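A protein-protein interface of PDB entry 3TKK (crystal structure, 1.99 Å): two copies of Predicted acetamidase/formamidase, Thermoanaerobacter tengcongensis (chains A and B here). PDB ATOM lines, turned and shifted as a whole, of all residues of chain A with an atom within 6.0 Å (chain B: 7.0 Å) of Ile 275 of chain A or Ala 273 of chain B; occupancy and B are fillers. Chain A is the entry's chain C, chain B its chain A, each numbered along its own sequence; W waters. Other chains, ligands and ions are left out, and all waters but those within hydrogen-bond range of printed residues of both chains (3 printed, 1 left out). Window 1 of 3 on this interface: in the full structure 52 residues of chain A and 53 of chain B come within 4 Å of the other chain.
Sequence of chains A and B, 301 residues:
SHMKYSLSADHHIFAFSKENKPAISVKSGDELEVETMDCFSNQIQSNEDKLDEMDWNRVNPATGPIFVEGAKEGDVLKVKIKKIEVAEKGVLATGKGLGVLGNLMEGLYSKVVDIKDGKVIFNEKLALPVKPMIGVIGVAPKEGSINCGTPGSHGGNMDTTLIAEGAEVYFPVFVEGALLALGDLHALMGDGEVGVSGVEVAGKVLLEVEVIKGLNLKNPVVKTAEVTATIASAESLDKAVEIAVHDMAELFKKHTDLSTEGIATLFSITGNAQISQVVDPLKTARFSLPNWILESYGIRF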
ATOM      1  N   THR A 161      -4.223  -2.894 -20.254  1.00  0.00           N
ATOM      2  CA  THR A 161      -4.931  -3.732 -21.224  1.00  0.00           C
ATOM      3  C   THR A 161      -5.198  -5.167 -20.745  1.00  0.00           C
ATOM      4  O   THR A 161      -6.053  -5.831 -21.307  1.00  0.00           O
ATOM      5  CB  THR A 161      -4.025  -3.970 -22.523  1.00  0.00           C
ATOM      6  OG1 THR A 161      -2.638  -4.151 -22.109  1.00  0.00           O
ATOM      7  CG2 THR A 161      -4.001  -2.743 -23.465  1.00  0.00           C
ATOM      8  N   GLY A 190      -4.407   0.782 -26.834  1.00  0.00           N
ATOM      9  CA  GLY A 190      -3.045   0.249 -26.917  1.00  0.00           C
ATOM     10  C   GLY A 190      -2.201   0.581 -25.741  1.00  0.00           C
ATOM     11  O   GLY A 190      -2.407   1.556 -25.056  1.00  0.00           O
ATOM     12  N   ASP A 191      -1.153  -0.177 -25.503  1.00  0.00           N
ATOM     13  CA  ASP A 191      -0.425   0.091 -24.296  1.00  0.00           C
ATOM     14  C   ASP A 191       0.194   1.516 -24.435  1.00  0.00           C
ATOM     15  O   ASP A 191       0.664   1.877 -25.489  1.00  0.00           O
ATOM     16  CB  ASP A 191       0.717  -0.889 -24.225  1.00  0.00           C
ATOM     17  CG  ASP A 191       0.415  -2.121 -23.429  1.00  0.00           C
ATOM     18  OD1 ASP A 191      -0.637  -2.196 -22.795  1.00  0.00           O
ATOM     19  OD2 ASP A 191       1.283  -3.051 -23.492  1.00  0.00           O
ATOM     20  N   GLY A 192       0.273   2.251 -23.331  1.00  0.00           N
ATOM     21  CA  GLY A 192       0.743   3.645 -23.387  1.00  0.00           C
ATOM     22  C   GLY A 192      -0.429   4.676 -23.509  1.00  0.00           C
ATOM     23  O   GLY A 192      -0.335   5.851 -22.977  1.00  0.00           O
ATOM     24  N   VAL A 194      -1.281   6.626 -25.861  1.00  0.00           N
ATOM     25  CA  VAL A 194      -0.445   7.827 -26.162  1.00  0.00           C
ATOM     26  C   VAL A 194      -1.176   9.009 -26.765  1.00  0.00           C
ATOM     27  O   VAL A 194      -0.646  10.148 -26.751  1.00  0.00           O
ATOM     28  CB  VAL A 194       0.806   7.458 -27.057  1.00  0.00           C
ATOM     29  CG1 VAL A 194       1.598   6.319 -26.347  1.00  0.00           C
ATOM     30  CG2 VAL A 194       0.354   6.991 -28.486  1.00  0.00           C
ATOM     31  N   LEU A 237       7.675   6.597 -15.700  1.00  0.00           N
ATOM     32  CA  LEU A 237       7.773   5.213 -16.034  1.00  0.00           C
ATOM     33  C   LEU A 237       8.923   4.535 -15.335  1.00  0.00           C
ATOM     34  O   LEU A 237       8.783   3.378 -14.925  1.00  0.00           O
ATOM     35  CB  LEU A 237       7.879   4.892 -17.574  1.00  0.00           C
ATOM     36  CG  LEU A 237       6.624   5.144 -18.375  1.00  0.00           C
ATOM     37  CD1 LEU A 237       6.961   4.812 -19.871  1.00  0.00           C
ATOM     38  CD2 LEU A 237       5.712   4.110 -17.770  1.00  0.00           C
ATOM     39  N   VAL A 241       8.304   1.275 -13.218  1.00  0.00           N
ATOM     40  CA  VAL A 241       8.928  -0.026 -13.473  1.00  0.00           C
ATOM     41  C   VAL A 241       9.697  -0.533 -12.284  1.00  0.00           C
ATOM     42  O   VAL A 241       9.603  -1.717 -11.928  1.00  0.00           O
ATOM     43  CB  VAL A 241       9.879   0.034 -14.759  1.00  0.00           C
ATOM     44  CG1 VAL A 241      10.672  -1.285 -14.939  1.00  0.00           C
ATOM     45  CG2 VAL A 241       9.025   0.393 -16.003  1.00  0.00           C
ATOM     46  N   ALA A 273       9.182  -6.223 -18.397  1.00  0.00           N
ATOM     47  CA  ALA A 273       8.634  -4.982 -18.061  1.00  0.00           C
ATOM     48  C   ALA A 273       7.823  -4.422 -19.269  1.00  0.00           C
ATOM     49  O   ALA A 273       8.296  -4.475 -20.408  1.00  0.00           O
ATOM     50  CB  ALA A 273       9.838  -3.960 -17.697  1.00  0.00           C
ATOM     51  N   GLN A 274       6.617  -3.941 -18.993  1.00  0.00           N
ATOM     52  CA  GLN A 274       5.746  -3.362 -19.941  1.00  0.00           C
ATOM     53  C   GLN A 274       5.094  -2.049 -19.477  1.00  0.00           C
ATOM     54  O   GLN A 274       5.201  -1.623 -18.348  1.00  0.00           O
ATOM     55  CB  GLN A 274       4.628  -4.359 -20.210  1.00  0.00           C
ATOM     56  CG  GLN A 274       5.271  -5.739 -20.493  1.00  0.00           C
ATOM     57  CD  GLN A 274       4.191  -6.844 -20.676  1.00  0.00           C
ATOM     58  OE1 GLN A 274       4.433  -7.800 -21.440  1.00  0.00           O
ATOM     59  NE2 GLN A 274       3.156  -6.817 -19.877  1.00  0.00           N
ATOM     60  N   ILE A 275       4.359  -1.424 -20.372  1.00  0.00           N
ATOM     61  CA  ILE A 275       3.802  -0.101 -20.066  1.00  0.00           C
ATOM     62  C   ILE A 275       2.306  -0.209 -20.212  1.00  0.00           C
ATOM     63  O   ILE A 275       1.801  -0.736 -21.195  1.00  0.00           O
ATOM     64  CB  ILE A 275       4.382   0.976 -21.072  1.00  0.00           C
ATOM     65  CG1 ILE A 275       5.874   1.201 -20.858  1.00  0.00           C
ATOM     66  CG2 ILE A 275       3.460   2.322 -21.174  1.00  0.00           C
ATOM     67  CD1 ILE A 275       6.561   1.921 -22.053  1.00  0.00           C
ATOM     68  N   SER A 276       1.604   0.356 -19.266  1.00  0.00           N
ATOM     69  CA  SER A 276       0.106   0.478 -19.329  1.00  0.00           C
ATOM     70  C   SER A 276      -0.302   1.798 -19.873  1.00  0.00           C
ATOM     71  O   SER A 276      -1.047   1.827 -20.822  1.00  0.00           O
ATOM     72  CB  SER A 276      -0.497   0.336 -17.934  1.00  0.00           C
ATOM     73  OG  SER A 276      -0.361  -1.004 -17.509  1.00  0.00           O
ATOM     74  N   GLN A 277       0.121   2.895 -19.230  1.00  0.00           N
ATOM     75  CA  GLN A 277      -0.273   4.202 -19.798  1.00  0.00           C
ATOM     76  C   GLN A 277       0.730   5.249 -19.448  1.00  0.00           C
ATOM     77  O   GLN A 277       1.302   5.232 -18.341  1.00  0.00           O
ATOM     78  CB  GLN A 277      -1.702   4.655 -19.345  1.00  0.00           C
ATOM     79  CG  GLN A 277      -1.975   4.792 -17.809  1.00  0.00           C
ATOM     80  CD  GLN A 277      -1.317   6.041 -17.196  1.00  0.00           C
ATOM     81  OE1 GLN A 277      -1.022   6.987 -17.921  1.00  0.00           O
ATOM     82  NE2 GLN A 277      -1.096   6.045 -15.848  1.00  0.00           N
ATOM     83  N   VAL A 278       0.931   6.190 -20.360  1.00  0.00           N
ATOM     84  CA  VAL A 278       1.876   7.241 -20.050  1.00  0.00           C
ATOM     85  C   VAL A 278       1.312   8.633 -19.978  1.00  0.00           C
ATOM     86  O   VAL A 278       2.060   9.595 -19.979  1.00  0.00           O
ATOM     87  CB  VAL A 278       3.109   7.219 -21.027  1.00  0.00           C
ATOM     88  CG1 VAL A 278       3.666   5.853 -21.061  1.00  0.00           C
ATOM     89  CG2 VAL A 278       2.700   7.640 -22.410  1.00  0.00           C
ATOM     90  N   THR A 284       1.772   4.477 -15.447  1.00  0.00           N
ATOM     91  CA  THR A 284       1.496   3.156 -14.915  1.00  0.00           C
ATOM     92  C   THR A 284       2.281   2.110 -15.725  1.00  0.00           C
ATOM     93  O   THR A 284       2.269   2.143 -16.967  1.00  0.00           O
ATOM     94  CB  THR A 284      -0.012   2.822 -14.947  1.00  0.00           C
ATOM     95  OG1 THR A 284      -0.739   3.731 -14.116  1.00  0.00           O
ATOM     96  CG2 THR A 284      -0.248   1.354 -14.428  1.00  0.00           C
ATOM     97  N   ALA A 285       3.012   1.220 -15.046  1.00  0.00           N
ATOM     98  CA  ALA A 285       3.765   0.161 -15.745  1.00  0.00           C
ATOM     99  C   ALA A 285       3.477  -1.181 -15.057  1.00  0.00           C
ATOM    100  O   ALA A 285       2.753  -1.215 -14.030  1.00  0.00           O
ATOM    101  CB  ALA A 285       5.255   0.394 -15.686  1.00  0.00           C
ATOM    102  N   ARG A 286       4.075  -2.251 -15.567  1.00  0.00           N
ATOM    103  CA  ARG A 286       3.833  -3.534 -15.015  1.00  0.00           C
ATOM    104  C   ARG A 286       4.981  -4.548 -15.264  1.00  0.00           C
ATOM    105  O   ARG A 286       5.805  -4.317 -16.148  1.00  0.00           O
ATOM    106  CB  ARG A 286       2.482  -3.993 -15.553  1.00  0.00           C
ATOM    107  CG  ARG A 286       2.468  -4.250 -16.964  1.00  0.00           C
ATOM    108  CD  ARG A 286       1.009  -4.576 -17.491  1.00  0.00           C
ATOM    109  NE  ARG A 286       1.186  -5.016 -18.885  1.00  0.00           N
ATOM    110  CZ  ARG A 286       0.808  -4.323 -19.992  1.00  0.00           C
ATOM    111  NH1 ARG A 286       0.127  -3.175 -19.837  1.00  0.00           N
ATOM    112  NH2 ARG A 286       0.977  -4.795 -21.277  1.00  0.00           N
ATOM    113  N   LEU B 237      13.113   6.371 -19.536  1.00  0.00           N
ATOM    114  CA  LEU B 237      12.120   5.643 -20.292  1.00  0.00           C
ATOM    115  C   LEU B 237      10.995   6.535 -20.795  1.00  0.00           C
ATOM    116  O   LEU B 237      10.548   6.360 -21.921  1.00  0.00           O
ATOM    117  CB  LEU B 237      11.482   4.625 -19.341  1.00  0.00           C
ATOM    118  CG  LEU B 237      11.152   3.267 -19.818  1.00  0.00           C
ATOM    119  CD1 LEU B 237      12.111   2.576 -20.874  1.00  0.00           C
ATOM    120  CD2 LEU B 237      10.922   2.279 -18.656  1.00  0.00           C
ATOM    121  N   VAL B 241      10.219   6.897 -24.631  1.00  0.00           N
ATOM    122  CA  VAL B 241       8.913   6.525 -25.233  1.00  0.00           C
ATOM    123  C   VAL B 241       8.380   7.705 -26.085  1.00  0.00           C
ATOM    124  O   VAL B 241       7.878   7.552 -27.243  1.00  0.00           O
ATOM    125  CB  VAL B 241       7.879   6.252 -24.102  1.00  0.00           C
ATOM    126  CG1 VAL B 241       6.422   6.437 -24.644  1.00  0.00           C
ATOM    127  CG2 VAL B 241       8.059   4.849 -23.465  1.00  0.00           C
ATOM    128  N   VAL B 245       7.389   7.495 -30.101  1.00  0.00           N
ATOM    129  CA  VAL B 245       6.065   7.876 -30.600  1.00  0.00           C
ATOM    130  C   VAL B 245       6.134   8.977 -31.614  1.00  0.00           C
ATOM    131  O   VAL B 245       5.505   8.885 -32.651  1.00  0.00           O
ATOM    132  CB  VAL B 245       5.154   8.292 -29.376  1.00  0.00           C
ATOM    133  CG1 VAL B 245       3.731   8.787 -29.736  1.00  0.00           C
ATOM    134  CG2 VAL B 245       5.011   7.110 -28.521  1.00  0.00           C
ATOM    135  N   PHE B 267      -2.922   5.844 -32.835  1.00  0.00           N
ATOM    136  CA  PHE B 267      -1.818   5.324 -32.058  1.00  0.00           C
ATOM    137  C   PHE B 267      -2.294   4.947 -30.638  1.00  0.00           C
ATOM    138  O   PHE B 267      -1.761   3.998 -30.036  1.00  0.00           O
ATOM    139  CB  PHE B 267      -0.784   6.401 -31.901  1.00  0.00           C
ATOM    140  CG  PHE B 267       0.140   6.561 -33.117  1.00  0.00           C
ATOM    141  CD1 PHE B 267      -0.188   6.031 -34.360  1.00  0.00           C
ATOM    142  CD2 PHE B 267       1.272   7.275 -32.995  1.00  0.00           C
ATOM    143  CE1 PHE B 267       0.672   6.175 -35.461  1.00  0.00           C
ATOM    144  CE2 PHE B 267       2.129   7.460 -34.082  1.00  0.00           C
ATOM    145  CZ  PHE B 267       1.818   6.887 -35.334  1.00  0.00           C
ATOM    146  N   GLY B 271      -1.578   1.233 -31.250  1.00  0.00           N
ATOM    147  CA  GLY B 271      -0.163   1.128 -31.077  1.00  0.00           C
ATOM    148  C   GLY B 271       0.221   0.867 -29.613  1.00  0.00           C
ATOM    149  O   GLY B 271      -0.523   1.228 -28.687  1.00  0.00           O
ATOM    150  N   ASN B 272       1.403   0.276 -29.400  1.00  0.00           N
ATOM    151  CA  ASN B 272       1.794  -0.247 -28.077  1.00  0.00           C
ATOM    152  C   ASN B 272       3.136   0.313 -27.733  1.00  0.00           C
ATOM    153  O   ASN B 272       4.157   0.004 -28.438  1.00  0.00           O
ATOM    154  CB  ASN B 272       1.855  -1.821 -28.105  1.00  0.00           C
ATOM    155  CG  ASN B 272       0.505  -2.444 -28.255  1.00  0.00           C
ATOM    156  OD1 ASN B 272      -0.356  -2.226 -27.442  1.00  0.00           O
ATOM    157  ND2 ASN B 272       0.315  -3.287 -29.278  1.00  0.00           N
ATOM    158  N   ALA B 273       3.185   1.177 -26.739  1.00  0.00           N
ATOM    159  CA  ALA B 273       4.480   1.618 -26.267  1.00  0.00           C
ATOM    160  C   ALA B 273       5.082   0.443 -25.474  1.00  0.00           C
ATOM    161  O   ALA B 273       4.371  -0.120 -24.679  1.00  0.00           O
ATOM    162  CB  ALA B 273       4.254   2.793 -25.381  1.00  0.00           C
ATOM    163  N   GLN B 274       6.381   0.135 -25.617  1.00  0.00           N
ATOM    164  CA  GLN B 274       6.908  -1.145 -25.068  1.00  0.00           C
ATOM    165  C   GLN B 274       8.309  -0.774 -24.590  1.00  0.00           C
ATOM    166  O   GLN B 274       8.845   0.319 -24.908  1.00  0.00           O
ATOM    167  CB  GLN B 274       6.941  -2.193 -26.171  1.00  0.00           C
ATOM    168  CG  GLN B 274       5.539  -2.518 -26.703  1.00  0.00           C
ATOM    169  CD  GLN B 274       5.525  -3.737 -27.608  1.00  0.00           C
ATOM    170  OE1 GLN B 274       6.504  -3.917 -28.340  1.00  0.00           O
ATOM    171  NE2 GLN B 274       4.411  -4.573 -27.609  1.00  0.00           N
ATOM    172  N   ILE B 275       8.856  -1.632 -23.738  1.00  0.00           N
ATOM    173  CA  ILE B 275      10.134  -1.416 -23.157  1.00  0.00           C
ATOM    174  C   ILE B 275      11.145  -2.442 -23.689  1.00  0.00           C
ATOM    175  O   ILE B 275      10.852  -3.711 -23.782  1.00  0.00           O
ATOM    176  CB  ILE B 275      10.024  -1.560 -21.602  1.00  0.00           C
ATOM    177  CG1 ILE B 275       9.269  -0.346 -20.975  1.00  0.00           C
ATOM    178  CG2 ILE B 275      11.417  -1.541 -20.915  1.00  0.00           C
ATOM    179  CD1 ILE B 275       8.793  -0.686 -19.526  1.00  0.00           C
ATOM    180  N   ALA B 285      13.228   2.155 -25.452  1.00  0.00           N
ATOM    181  CA  ALA B 285      11.851   1.853 -25.562  1.00  0.00           C
ATOM    182  C   ALA B 285      11.482   1.766 -26.980  1.00  0.00           C
ATOM    183  O   ALA B 285      12.284   2.098 -27.876  1.00  0.00           O
ATOM    184  CB  ALA B 285      10.971   3.045 -24.920  1.00  0.00           C
ATOM    185  N   ARG B 286      10.247   1.364 -27.195  1.00  0.00           N
ATOM    186  CA  ARG B 286       9.801   1.284 -28.520  1.00  0.00           C
ATOM    187  C   ARG B 286       8.363   1.613 -28.710  1.00  0.00           C
ATOM    188  O   ARG B 286       7.608   1.604 -27.741  1.00  0.00           O
ATOM    189  CB  ARG B 286      10.155  -0.054 -29.096  1.00  0.00           C
ATOM    190  CG  ARG B 286       9.536  -1.228 -28.516  1.00  0.00           C
ATOM    191  CD  ARG B 286      10.306  -2.513 -28.908  1.00  0.00           C
ATOM    192  NE  ARG B 286       9.461  -3.614 -28.414  1.00  0.00           N
ATOM    193  CZ  ARG B 286       9.738  -4.399 -27.359  1.00  0.00           C
ATOM    194  NH1 ARG B 286      10.953  -4.420 -26.842  1.00  0.00           N
ATOM    195  NH2 ARG B 286       8.864  -5.376 -27.010  1.00  0.00           N
ATOM    196  N   PHE B 287       7.961   1.946 -29.935  1.00  0.00           N
ATOM    197  CA  PHE B 287       6.508   2.011 -30.230  1.00  0.00           C
ATOM    198  C   PHE B 287       6.076   1.150 -31.407  1.00  0.00           C
ATOM    199  O   PHE B 287       6.561   1.297 -32.523  1.00  0.00           O
ATOM    200  CB  PHE B 287       6.105   3.479 -30.444  1.00  0.00           C
ATOM    201  CG  PHE B 287       4.598   3.655 -30.565  1.00  0.00           C
ATOM    202  CD1 PHE B 287       3.803   3.550 -29.432  1.00  0.00           C
ATOM    203  CD2 PHE B 287       4.010   4.022 -31.780  1.00  0.00           C
ATOM    204  CE1 PHE B 287       2.428   3.662 -29.487  1.00  0.00           C
ATOM    205  CE2 PHE B 287       2.591   4.155 -31.821  1.00  0.00           C
ATOM    206  CZ  PHE B 287       1.816   4.048 -30.684  1.00  0.00           C
ATOM    207  N   SER B 288       5.123   0.241 -31.190  1.00  0.00           N
ATOM    208  CA  SER B 288       4.922  -0.817 -32.149  1.00  0.00           C
ATOM    209  C   SER B 288       3.518  -0.696 -32.697  1.00  0.00           C
ATOM    210  O   SER B 288       2.568  -0.607 -31.900  1.00  0.00           O
ATOM    211  CB  SER B 288       4.982  -2.078 -31.314  1.00  0.00           C
ATOM    212  OG  SER B 288       4.809  -3.230 -32.031  1.00  0.00           O
HETATM  213  O   HOH W   1       2.228  -4.241 -25.811  1.00  0.00           O
HETATM  214  O   HOH W   2       7.700  -4.175 -23.040  1.00  0.00           O
HETATM  215  O   HOH W   3       3.960  -2.364 -23.081  1.00  0.00           O
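The backbone NH of Asp 191 of chain A sits at hydrogen-bond distance from the side-chain amide oxygen of Asn 272 of chain B (2.9 Å).
O of Asp 191 of chain A lies close to O of Gly 271 of chain B (3.5 Å).
O of Asp 191 of chain A sits at hydrogen-bond distance from N of Ala 273 of chain B, at 2.9 Å.
The side-chain carboxylate (OD2) of Asp 191 of chain A is in salt-bridge range of the guanidinium group (NH2) of Arg 286 of chain A, at 2.8 Å.
The backbone carbonyl oxygen (O) of Ile 275 of chain A is in hydrogen-bond range of the guanidinium group (NH1) of Arg 286 of chain A, at 3.3 Å.
The backbone carbonyl oxygen (O) of Arg 286 of chain B is in hydrogen-bond range of the backbone NH (N) of Gln 274 of chain B, at 2.9 Å.
The backbone carbonyl oxygen (O) of Ser 288 of chain B sits at hydrogen-bond distance from the backbone NH (N) of Asn 272 of chain B, at 2.9 Å.
OG1 of Thr 161 of chain A is in hydrogen-bond range of OD1 of Asp 191 of chain A (2.9 Å).
The guanidinium group of Arg 286 of chain A sits close to the side-chain amide nitrogen of Gln 274 of chain A (2.8 Å).
Among the printed residues, pairs that only touch across the chains: Gly 190 of chain A with Gly 271 of chain B (3.2 Å), Gly 190 of chain A with Asn 272 of chain B (3.7 Å), Val 194 of chain A with Phe 267 of chain B (3.6 Å), Val 194 of chain A with Phe 287 of chain B (3.95 Å), Leu 237 of chain A with Val 241 of chain B (3.8 Å), Val 241 of chain A with Leu 237 of chain B (3.8 Å), Val 241 of chain A with Ile 275 of chain B (3.7 Å), Ala 273 of chain A with Ile 275 of chain B (3.6 Å), Gln 274 of chain A with Ile 275 of chain B (3.9 Å), Ile 275 of chain A with Val 241 of chain B (3.6 Å), Ile 275 of chain A with Ala 273 of chain B (3.8 Å), Ile 275 of chain A with Gln 274 of chain B (3.99 Å) and Ile 275 of chain A with Ile 275 of chain B (3.7 Å).
Of the printed residues of chain B, Gly 190 of chain A touches Gly 271 and Asn 272.
Printed residues of chain B within 4 Å of Ile 275 of chain A: Val 241 (3.6 Å), Ala 273 (3.8 Å), Gln 274 (3.99 Å) and Ile 275 (3.7 Å).
Of the printed residues of chain A, Asn 272 of chain B touches Gly 190 and Asp 191.
Ala 273 of chain B touches just these residues of chain A: Asp 191 and Ile 275.
Of the printed residues of chain A, Gln 274 of chain B touches Ile 275.
Of the 13 printed residues of chain B, 9 touch a printed residue of chain A.
Printed residues of chain B that touch a printed residue of chain A: Leu 237, Val 241, Phe 267, Gly 271, Asn 272, Ala 273, Gln 274, Ile 275 and Phe 287.
Hydrophobic or aromatic side chains of chain B within 4 Å of the printed part of chain A: Leu 237, Val 241, Phe 267, Ala 273, Ile 275 and Phe 287.
Of the 16 printed residues of chain A, 8 touch a printed residue of chain B.
Among the printed residues, 16 pairs touch across the chains.
Leu 237 of chain A touches Val 241 of chain B, and with the chains exchanged Val 241 of chain A touches Leu 237 of chain B.
Val 241 of chain A touches Ile 275 of chain B, and with the chains exchanged Ile 275 of chain A touches Val 241 of chain B.
Ala 273 of chain A touches Ile 275 of chain B, and with the chains exchanged Ile 275 of chain A touches Ala 273 of chain B.
Gln 274 of chain A touches Ile 275 of chain B, and with the chains exchanged Ile 275 of chain A touches Gln 274 of chain B.
Positions printed for both chains: 237, 241, 273, 274, 275, 285 and 286.
Of the 16 pairs that touch across the chains among the printed residues, 9 have their exchanged pair printed and touching as well.
Water W2 bridges the backbone carbonyl oxygen (O) of Ala 273 of chain A and the backbone NH (N) of Ile 275 of chain B.
Water W1 bridges the side-chain carboxylate (OD2) of Asp 191 of chain A and the side-chain amide nitrogen (NE2) of Gln 274 of chain B.
Water W3 lies within hydrogen-bond range of O of Ala 273 of chain B, OD2 of Asp 191 of chain A and N of Ile 275 of chain A.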
